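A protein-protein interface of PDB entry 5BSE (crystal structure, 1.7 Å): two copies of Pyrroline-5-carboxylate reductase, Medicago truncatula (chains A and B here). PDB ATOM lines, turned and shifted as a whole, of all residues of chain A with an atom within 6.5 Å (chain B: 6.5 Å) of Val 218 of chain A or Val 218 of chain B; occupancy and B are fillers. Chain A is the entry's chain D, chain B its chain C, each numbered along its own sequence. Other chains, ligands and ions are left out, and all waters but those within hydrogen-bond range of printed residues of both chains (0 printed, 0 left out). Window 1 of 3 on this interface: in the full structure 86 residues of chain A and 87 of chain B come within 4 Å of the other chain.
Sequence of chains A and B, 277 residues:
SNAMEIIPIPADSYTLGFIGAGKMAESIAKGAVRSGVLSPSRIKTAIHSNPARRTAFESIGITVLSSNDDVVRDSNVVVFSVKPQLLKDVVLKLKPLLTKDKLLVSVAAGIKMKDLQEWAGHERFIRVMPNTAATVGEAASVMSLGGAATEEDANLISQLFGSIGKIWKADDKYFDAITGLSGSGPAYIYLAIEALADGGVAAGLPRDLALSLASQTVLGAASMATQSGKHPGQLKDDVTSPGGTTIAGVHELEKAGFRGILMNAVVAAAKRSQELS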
ATOM      1  N   GLY A 185      20.034 -19.254  -4.250  1.00  0.00           N
ATOM      2  CA  GLY A 185      19.318 -20.195  -5.095  1.00  0.00           C
ATOM      3  C   GLY A 185      20.141 -21.263  -5.716  1.00  0.00           C
ATOM      4  O   GLY A 185      19.689 -22.380  -5.883  1.00  0.00           O
ATOM      5  N   PRO A 186      21.406 -20.985  -6.064  1.00  0.00           N
ATOM      6  CA  PRO A 186      22.148 -22.117  -6.688  1.00  0.00           C
ATOM      7  C   PRO A 186      22.309 -23.330  -5.783  1.00  0.00           C
ATOM      8  O   PRO A 186      22.195 -24.419  -6.279  1.00  0.00           O
ATOM      9  CB  PRO A 186      23.521 -21.483  -7.002  1.00  0.00           C
ATOM     10  CG  PRO A 186      23.180 -20.025  -7.246  1.00  0.00           C
ATOM     11  CD  PRO A 186      22.099 -19.700  -6.217  1.00  0.00           C
ATOM     12  N   ILE A 189      19.315 -25.565  -6.159  1.00  0.00           N
ATOM     13  CA  ILE A 189      19.402 -26.305  -7.381  1.00  0.00           C
ATOM     14  C   ILE A 189      20.444 -27.396  -7.297  1.00  0.00           C
ATOM     15  O   ILE A 189      20.253 -28.465  -7.870  1.00  0.00           O
ATOM     16  CB  ILE A 189      19.601 -25.322  -8.534  1.00  0.00           C
ATOM     17  CG1 ILE A 189      18.430 -24.399  -8.590  1.00  0.00           C
ATOM     18  CG2 ILE A 189      19.724 -26.100  -9.843  1.00  0.00           C
ATOM     19  CD1 ILE A 189      17.034 -24.994  -8.555  1.00  0.00           C
ATOM     20  N   ALA A 192      18.640 -29.998  -5.683  1.00  0.00           N
ATOM     21  CA  ALA A 192      17.738 -30.563  -6.618  1.00  0.00           C
ATOM     22  C   ALA A 192      18.365 -31.535  -7.621  1.00  0.00           C
ATOM     23  O   ALA A 192      17.811 -32.579  -7.904  1.00  0.00           O
ATOM     24  CB  ALA A 192      16.974 -29.513  -7.371  1.00  0.00           C
ATOM     25  N   ILE A 193      19.526 -31.156  -8.125  1.00  0.00           N
ATOM     26  CA  ILE A 193      20.258 -32.017  -9.076  1.00  0.00           C
ATOM     27  C   ILE A 193      20.692 -33.298  -8.392  1.00  0.00           C
ATOM     28  O   ILE A 193      20.444 -34.403  -8.978  1.00  0.00           O
ATOM     29  CB  ILE A 193      21.424 -31.267  -9.646  1.00  0.00           C
ATOM     30  CG1 ILE A 193      20.896 -30.231 -10.641  1.00  0.00           C
ATOM     31  CG2 ILE A 193      22.392 -32.263 -10.330  1.00  0.00           C
ATOM     32  CD1 ILE A 193      22.002 -29.231 -11.058  1.00  0.00           C
ATOM     33  N   LEU A 196      17.514 -35.410  -7.891  1.00  0.00           N
ATOM     34  CA  LEU A 196      17.017 -35.943  -9.149  1.00  0.00           C
ATOM     35  C   LEU A 196      17.870 -37.125  -9.556  1.00  0.00           C
ATOM     36  O   LEU A 196      17.354 -38.191  -9.977  1.00  0.00           O
ATOM     37  CB  LEU A 196      17.051 -34.890 -10.258  1.00  0.00           C
ATOM     38  CG  LEU A 196      15.940 -33.822 -10.164  1.00  0.00           C
ATOM     39  CD1 LEU A 196      16.259 -32.716 -11.068  1.00  0.00           C
ATOM     40  CD2 LEU A 196      14.595 -34.477 -10.399  1.00  0.00           C
ATOM     41  N   LEU A 213      22.156 -36.827 -16.633  1.00  0.00           N
ATOM     42  CA  LEU A 213      20.808 -36.455 -17.040  1.00  0.00           C
ATOM     43  C   LEU A 213      20.224 -35.385 -16.179  1.00  0.00           C
ATOM     44  O   LEU A 213      19.530 -34.488 -16.634  1.00  0.00           O
ATOM     45  CB  LEU A 213      19.889 -37.662 -17.088  1.00  0.00           C
ATOM     46  CG  LEU A 213      20.171 -38.682 -18.189  1.00  0.00           C
ATOM     47  CD1 LEU A 213      19.217 -39.836 -18.013  1.00  0.00           C
ATOM     48  CD2 LEU A 213      20.033 -38.092 -19.570  1.00  0.00           C
ATOM     49  N   ALA A 214      20.420 -35.529 -14.898  1.00  0.00           N
ATOM     50  CA  ALA A 214      19.828 -34.562 -13.942  1.00  0.00           C
ATOM     51  C   ALA A 214      20.314 -33.186 -14.215  1.00  0.00           C
ATOM     52  O   ALA A 214      19.545 -32.232 -14.367  1.00  0.00           O
ATOM     53  CB  ALA A 214      20.108 -34.956 -12.545  1.00  0.00           C
ATOM     54  N   SER A 215      21.669 -33.042 -14.333  1.00  0.00           N
ATOM     55  CA  SER A 215      22.219 -31.728 -14.573  1.00  0.00           C
ATOM     56  C   SER A 215      21.756 -31.123 -15.874  1.00  0.00           C
ATOM     57  O   SER A 215      21.358 -29.958 -15.982  1.00  0.00           O
ATOM     58  CB  SER A 215      23.767 -31.790 -14.573  1.00  0.00           C
ATOM     59  OG  SER A 215      24.129 -32.133 -13.256  1.00  0.00           O
ATOM     60  N   GLN A 216      21.760 -31.926 -16.959  1.00  0.00           N
ATOM     61  CA  GLN A 216      21.385 -31.409 -18.246  1.00  0.00           C
ATOM     62  C   GLN A 216      19.870 -31.141 -18.382  1.00  0.00           C
ATOM     63  O   GLN A 216      19.433 -30.253 -19.068  1.00  0.00           O
ATOM     64  CB  GLN A 216      21.809 -32.418 -19.346  1.00  0.00           C
ATOM     65  CG  GLN A 216      21.500 -31.926 -20.761  1.00  0.00           C
ATOM     66  CD  GLN A 216      22.268 -30.673 -21.099  1.00  0.00           C
ATOM     67  OE1 GLN A 216      23.360 -30.387 -20.644  1.00  0.00           O
ATOM     68  NE2 GLN A 216      21.629 -29.856 -21.938  1.00  0.00           N
ATOM     69  N   THR A 217      19.068 -31.948 -17.655  1.00  0.00           N
ATOM     70  CA  THR A 217      17.618 -31.702 -17.599  1.00  0.00           C
ATOM     71  C   THR A 217      17.299 -30.374 -16.937  1.00  0.00           C
ATOM     72  O   THR A 217      16.504 -29.571 -17.473  1.00  0.00           O
ATOM     73  CB  THR A 217      16.913 -32.860 -16.873  1.00  0.00           C
ATOM     74  OG1 THR A 217      17.119 -34.039 -17.656  1.00  0.00           O
ATOM     75  CG2 THR A 217      15.480 -32.603 -16.727  1.00  0.00           C
ATOM     76  N   VAL A 218      17.984 -30.089 -15.842  1.00  0.00           N
ATOM     77  CA  VAL A 218      17.827 -28.782 -15.183  1.00  0.00           C
ATOM     78  C   VAL A 218      18.251 -27.660 -16.144  1.00  0.00           C
ATOM     79  O   VAL A 218      17.586 -26.612 -16.266  1.00  0.00           O
ATOM     80  CB  VAL A 218      18.478 -28.734 -13.843  1.00  0.00           C
ATOM     81  CG1 VAL A 218      18.308 -27.384 -13.188  1.00  0.00           C
ATOM     82  CG2 VAL A 218      17.948 -29.832 -12.957  1.00  0.00           C
ATOM     83  N   LEU A 219      19.418 -27.831 -16.766  1.00  0.00           N
ATOM     84  CA  LEU A 219      19.945 -26.809 -17.660  1.00  0.00           C
ATOM     85  C   LEU A 219      18.929 -26.555 -18.786  1.00  0.00           C
ATOM     86  O   LEU A 219      18.617 -25.413 -19.122  1.00  0.00           O
ATOM     87  CB  LEU A 219      21.286 -27.261 -18.199  1.00  0.00           C
ATOM     88  CG  LEU A 219      21.949 -26.342 -19.242  1.00  0.00           C
ATOM     89  CD1 LEU A 219      22.029 -25.035 -18.643  1.00  0.00           C
ATOM     90  CD2 LEU A 219      23.365 -26.841 -19.464  1.00  0.00           C
ATOM     91  N   GLY A 220      18.452 -27.625 -19.403  1.00  0.00           N
ATOM     92  CA  GLY A 220      17.539 -27.490 -20.504  1.00  0.00           C
ATOM     93  C   GLY A 220      16.260 -26.822 -20.135  1.00  0.00           C
ATOM     94  O   GLY A 220      15.753 -25.965 -20.832  1.00  0.00           O
ATOM     95  N   ALA A 221      15.714 -27.183 -18.988  1.00  0.00           N
ATOM     96  CA  ALA A 221      14.435 -26.597 -18.571  1.00  0.00           C
ATOM     97  C   ALA A 221      14.606 -25.090 -18.291  1.00  0.00           C
ATOM     98  O   ALA A 221      13.794 -24.280 -18.669  1.00  0.00           O
ATOM     99  CB  ALA A 221      13.941 -27.280 -17.295  1.00  0.00           C
ATOM    100  N   ALA A 222      15.741 -24.747 -17.676  1.00  0.00           N
ATOM    101  CA  ALA A 222      16.027 -23.320 -17.359  1.00  0.00           C
ATOM    102  C   ALA A 222      16.195 -22.549 -18.641  1.00  0.00           C
ATOM    103  O   ALA A 222      15.746 -21.435 -18.768  1.00  0.00           O
ATOM    104  CB  ALA A 222      17.149 -23.141 -16.444  1.00  0.00           C
ATOM    105  N   SER A 223      16.835 -23.223 -19.580  1.00  0.00           N
ATOM    106  CA  SER A 223      17.009 -22.580 -20.917  1.00  0.00           C
ATOM    107  C   SER A 223      15.741 -22.354 -21.627  1.00  0.00           C
ATOM    108  O   SER A 223      15.515 -21.316 -22.288  1.00  0.00           O
ATOM    109  CB  SER A 223      17.924 -23.400 -21.795  1.00  0.00           C
ATOM    110  OG  SER A 223      19.175 -23.584 -21.170  1.00  0.00           O
ATOM    111  N   GLY B 185      11.439 -34.539 -15.987  1.00  0.00           N
ATOM    112  CA  GLY B 185      12.101 -33.589 -15.180  1.00  0.00           C
ATOM    113  C   GLY B 185      11.929 -32.125 -15.492  1.00  0.00           C
ATOM    114  O   GLY B 185      11.936 -31.304 -14.610  1.00  0.00           O
ATOM    115  N   PRO B 186      11.827 -31.755 -16.788  1.00  0.00           N
ATOM    116  CA  PRO B 186      11.700 -30.341 -17.028  1.00  0.00           C
ATOM    117  C   PRO B 186      10.511 -29.752 -16.352  1.00  0.00           C
ATOM    118  O   PRO B 186      10.588 -28.630 -15.854  1.00  0.00           O
ATOM    119  CB  PRO B 186      11.589 -30.250 -18.564  1.00  0.00           C
ATOM    120  CG  PRO B 186      12.388 -31.426 -19.003  1.00  0.00           C
ATOM    121  CD  PRO B 186      12.087 -32.514 -18.033  1.00  0.00           C
ATOM    122  N   ILE B 189      11.280 -28.706 -12.852  1.00  0.00           N
ATOM    123  CA  ILE B 189      12.057 -27.459 -12.836  1.00  0.00           C
ATOM    124  C   ILE B 189      11.202 -26.246 -13.210  1.00  0.00           C
ATOM    125  O   ILE B 189      11.432 -25.185 -12.656  1.00  0.00           O
ATOM    126  CB  ILE B 189      13.282 -27.656 -13.704  1.00  0.00           C
ATOM    127  CG1 ILE B 189      14.135 -28.827 -13.199  1.00  0.00           C
ATOM    128  CG2 ILE B 189      14.099 -26.375 -13.757  1.00  0.00           C
ATOM    129  CD1 ILE B 189      14.482 -28.766 -11.740  1.00  0.00           C
ATOM    130  N   ALA B 192       9.714 -25.455 -10.030  1.00  0.00           N
ATOM    131  CA  ALA B 192      10.742 -24.865  -9.159  1.00  0.00           C
ATOM    132  C   ALA B 192      10.968 -23.414  -9.499  1.00  0.00           C
ATOM    133  O   ALA B 192      11.142 -22.591  -8.623  1.00  0.00           O
ATOM    134  CB  ALA B 192      12.028 -25.637  -9.263  1.00  0.00           C
ATOM    135  N   ILE B 193      11.081 -23.123 -10.798  1.00  0.00           N
ATOM    136  CA  ILE B 193      11.268 -21.721 -11.271  1.00  0.00           C
ATOM    137  C   ILE B 193      10.140 -20.839 -10.824  1.00  0.00           C
ATOM    138  O   ILE B 193      10.360 -19.729 -10.274  1.00  0.00           O
ATOM    139  CB  ILE B 193      11.519 -21.694 -12.778  1.00  0.00           C
ATOM    140  CG1 ILE B 193      12.938 -22.254 -13.023  1.00  0.00           C
ATOM    141  CG2 ILE B 193      11.382 -20.265 -13.255  1.00  0.00           C
ATOM    142  CD1 ILE B 193      13.151 -22.506 -14.476  1.00  0.00           C
ATOM    143  N   LEU B 196      10.371 -20.373  -7.019  1.00  0.00           N
ATOM    144  CA  LEU B 196      11.426 -19.466  -6.630  1.00  0.00           C
ATOM    145  C   LEU B 196      11.035 -18.025  -6.903  1.00  0.00           C
ATOM    146  O   LEU B 196      11.263 -17.146  -6.085  1.00  0.00           O
ATOM    147  CB  LEU B 196      12.676 -19.832  -7.427  1.00  0.00           C
ATOM    148  CG  LEU B 196      13.424 -21.114  -6.926  1.00  0.00           C
ATOM    149  CD1 LEU B 196      14.466 -21.492  -7.969  1.00  0.00           C
ATOM    150  CD2 LEU B 196      13.988 -20.882  -5.575  1.00  0.00           C
ATOM    151  N   LEU B 213      15.319 -13.561 -12.386  1.00  0.00           N
ATOM    152  CA  LEU B 213      16.347 -14.054 -11.492  1.00  0.00           C
ATOM    153  C   LEU B 213      16.208 -15.560 -11.271  1.00  0.00           C
ATOM    154  O   LEU B 213      17.157 -16.295 -11.265  1.00  0.00           O
ATOM    155  CB  LEU B 213      16.384 -13.353 -10.172  1.00  0.00           C
ATOM    156  CG  LEU B 213      16.853 -11.874 -10.186  1.00  0.00           C
ATOM    157  CD1 LEU B 213      16.754 -11.303  -8.787  1.00  0.00           C
ATOM    158  CD2 LEU B 213      18.255 -11.774 -10.695  1.00  0.00           C
ATOM    159  N   ALA B 214      14.973 -15.987 -11.067  1.00  0.00           N
ATOM    160  CA  ALA B 214      14.740 -17.410 -10.805  1.00  0.00           C
ATOM    161  C   ALA B 214      15.238 -18.262 -11.963  1.00  0.00           C
ATOM    162  O   ALA B 214      15.982 -19.215 -11.816  1.00  0.00           O
ATOM    163  CB  ALA B 214      13.275 -17.689 -10.534  1.00  0.00           C
ATOM    164  N   SER B 215      14.832 -17.886 -13.202  1.00  0.00           N
ATOM    165  CA  SER B 215      15.230 -18.677 -14.354  1.00  0.00           C
ATOM    166  C   SER B 215      16.716 -18.695 -14.582  1.00  0.00           C
ATOM    167  O   SER B 215      17.315 -19.719 -14.813  1.00  0.00           O
ATOM    168  CB  SER B 215      14.533 -18.155 -15.624  1.00  0.00           C
ATOM    169  OG  SER B 215      13.155 -18.340 -15.476  1.00  0.00           O
ATOM    170  N   GLN B 216      17.324 -17.536 -14.442  1.00  0.00           N
ATOM    171  CA  GLN B 216      18.758 -17.467 -14.650  1.00  0.00           C
ATOM    172  C   GLN B 216      19.547 -18.119 -13.563  1.00  0.00           C
ATOM    173  O   GLN B 216      20.654 -18.642 -13.803  1.00  0.00           O
ATOM    174  CB  GLN B 216      19.156 -15.997 -14.811  1.00  0.00           C
ATOM    175  CG  GLN B 216      20.665 -15.786 -15.122  1.00  0.00           C
ATOM    176  CD  GLN B 216      21.065 -16.425 -16.463  1.00  0.00           C
ATOM    177  OE1 GLN B 216      20.294 -16.486 -17.434  1.00  0.00           O
ATOM    178  NE2 GLN B 216      22.255 -16.957 -16.508  1.00  0.00           N
ATOM    179  N   THR B 217      19.054 -18.056 -12.344  1.00  0.00           N
ATOM    180  CA  THR B 217      19.719 -18.711 -11.200  1.00  0.00           C
ATOM    181  C   THR B 217      19.765 -20.188 -11.477  1.00  0.00           C
ATOM    182  O   THR B 217      20.754 -20.865 -11.245  1.00  0.00           O
ATOM    183  CB  THR B 217      19.021 -18.340  -9.909  1.00  0.00           C
ATOM    184  OG1 THR B 217      19.196 -16.930  -9.692  1.00  0.00           O
ATOM    185  CG2 THR B 217      19.569 -19.056  -8.713  1.00  0.00           C
ATOM    186  N   VAL B 218      18.605 -20.754 -11.869  1.00  0.00           N
ATOM    187  CA  VAL B 218      18.560 -22.188 -12.147  1.00  0.00           C
ATOM    188  C   VAL B 218      19.511 -22.548 -13.304  1.00  0.00           C
ATOM    189  O   VAL B 218      20.242 -23.523 -13.271  1.00  0.00           O
ATOM    190  CB  VAL B 218      17.138 -22.682 -12.428  1.00  0.00           C
ATOM    191  CG1 VAL B 218      17.124 -24.140 -12.752  1.00  0.00           C
ATOM    192  CG2 VAL B 218      16.287 -22.371 -11.246  1.00  0.00           C
ATOM    193  N   LEU B 219      19.461 -21.732 -14.361  1.00  0.00           N
ATOM    194  CA  LEU B 219      20.341 -21.967 -15.536  1.00  0.00           C
ATOM    195  C   LEU B 219      21.810 -21.972 -15.079  1.00  0.00           C
ATOM    196  O   LEU B 219      22.582 -22.831 -15.456  1.00  0.00           O
ATOM    197  CB  LEU B 219      20.089 -20.911 -16.611  1.00  0.00           C
ATOM    198  CG  LEU B 219      20.978 -20.934 -17.845  1.00  0.00           C
ATOM    199  CD1 LEU B 219      20.825 -22.252 -18.388  1.00  0.00           C
ATOM    200  CD2 LEU B 219      20.404 -19.921 -18.857  1.00  0.00           C
ATOM    201  N   GLY B 220      22.176 -20.966 -14.305  1.00  0.00           N
ATOM    202  CA  GLY B 220      23.563 -20.850 -13.874  1.00  0.00           C
ATOM    203  C   GLY B 220      24.027 -21.945 -13.014  1.00  0.00           C
ATOM    204  O   GLY B 220      25.104 -22.511 -13.181  1.00  0.00           O
ATOM    205  N   ALA B 221      23.169 -22.350 -12.089  1.00  0.00           N
ATOM    206  CA  ALA B 221      23.529 -23.489 -11.222  1.00  0.00           C
ATOM    207  C   ALA B 221      23.697 -24.760 -12.032  1.00  0.00           C
ATOM    208  O   ALA B 221      24.630 -25.537 -11.784  1.00  0.00           O
ATOM    209  CB  ALA B 221      22.469 -23.668 -10.142  1.00  0.00           C
ATOM    210  N   ALA B 222      22.776 -25.005 -12.974  1.00  0.00           N
ATOM    211  CA  ALA B 222      22.856 -26.190 -13.793  1.00  0.00           C
ATOM    212  C   ALA B 222      24.107 -26.175 -14.643  1.00  0.00           C
ATOM    213  O   ALA B 222      24.788 -27.178 -14.823  1.00  0.00           O
ATOM    214  CB  ALA B 222      21.662 -26.405 -14.611  1.00  0.00           C
ATOM    215  N   SER B 223      24.418 -24.997 -15.118  1.00  0.00           N
ATOM    216  CA  SER B 223      25.677 -24.821 -15.890  1.00  0.00           C
ATOM    217  C   SER B 223      26.912 -25.048 -15.087  1.00  0.00           C
ATOM    218  O   SER B 223      27.901 -25.687 -15.553  1.00  0.00           O
ATOM    219  CB  SER B 223      25.765 -23.403 -16.494  1.00  0.00           C
ATOM    220  OG  SER B 223      24.658 -23.175 -17.297  1.00  0.00           O
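Of chain B, only Ile 189 (3.8 Å), Val 218 (3.5 Å) and Ala 222 (3.8 Å) come within 4 Å of Val 218 of chain A.
Val 218 of chain B touches just these residues of chain A: Ile 189, Val 218 and Ala 222.
Of the printed residues of chain A, Gly 185 of chain B touches Thr 217.
Printed residues of chain A within 4 Å of Ala 221 of chain B: Pro 186 and Ile 189.
The nearest residue of chain B that does not touch Val 218 of chain A is Leu 219 of chain B (5.4 Å).
Hydrophobic or aromatic side chains of chain B that line the printed part of chain A: Pro 186, Ile 189, Val 218, Leu 219, Ala 221 and Ala 222.
Of the 17 printed residues of chain A, 10 touch a printed residue of chain B.
Among the printed residues, no Asp or Glu carboxylate lies within 4 Å of a Lys or Arg side-chain nitrogen of the other chain.
OG1 of Thr 217 of chain B lies within hydrogen-bond range of O of Leu 213 of chain B (2.7 Å).
The side-chain hydroxyl of Ser 223 of chain B lies within hydrogen-bond range of the backbone carbonyl oxygen of Leu 219 of chain B, at 2.8 Å.
The backbone carbonyl oxygen of Leu 213 of chain A lies within hydrogen-bond range of the side-chain hydroxyl of Thr 217 of chain A (2.7 Å).
The backbone carbonyl oxygen (O) of Leu 219 of chain A sits at hydrogen-bond distance from the side-chain hydroxyl (OG) of Ser 223 of chain A.
Pro 186 of chain A touches Thr 217 of chain B, and with the chains exchanged Thr 217 of chain A touches Pro 186 of chain B.
Ile 189 of chain A touches Val 218 of chain B, and with the chains exchanged Val 218 of chain A touches Ile 189 of chain B.
Ile 189 of chain A touches Ala 221 of chain B, and with the chains exchanged Ala 221 of chain A touches Ile 189 of chain B.
Val 218 of chain B touches its own counterpart, Val 218 of chain A.
Of the 20 pairs that touch across the chains among the printed residues, 20 have their exchanged pair printed and touching as well.
Among the printed residues, pairs that only touch across the chains: Gly 185 of chain A with Thr 217 of chain B (3.8 Å), Pro 186 of chain A with Thr 217 of chain B (3.6 Å), Pro 186 of chain A with Ala 221 of chain B (3.8 Å), Ile 189 of chain A with Val 218 of chain B (3.8 Å), Ile 189 of chain A with Ala 221 of chain B (3.7 Å), Ser 215 of chain A with Ala 222 of chain B (3.8 Å), Thr 217 of chain A with Gly 185 of chain B (3.8 Å), Thr 217 of chain A with Pro 186 of chain B (3.6 Å), Val 218 of chain A with Ile 189 of chain B (3.8 Å), Val 218 of chain A with Val 218 of chain B (3.5 Å), Val 218 of chain A with Ala 222 of chain B (3.8 Å), Leu 219 of chain A with Leu 219 of chain B (3.0 Å), Leu 219 of chain A with Ala 222 of chain B (3.4 Å), Leu 219 of chain A with Ser 223 of chain B (3.5 Å), Ala 221 of chain A with Pro 186 of chain B (3.8 Å), Ala 221 of chain A with Ile 189 of chain B (3.7 Å), Ala 222 of chain A with Ser 215 of chain B (3.8 Å), Ala 222 of chain A with Val 218 of chain B (3.8 Å), Ala 222 of chain A with Leu 219 of chain B (3.4 Å) and Ser 223 of chain A with Leu 219 of chain B (3.5 Å).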
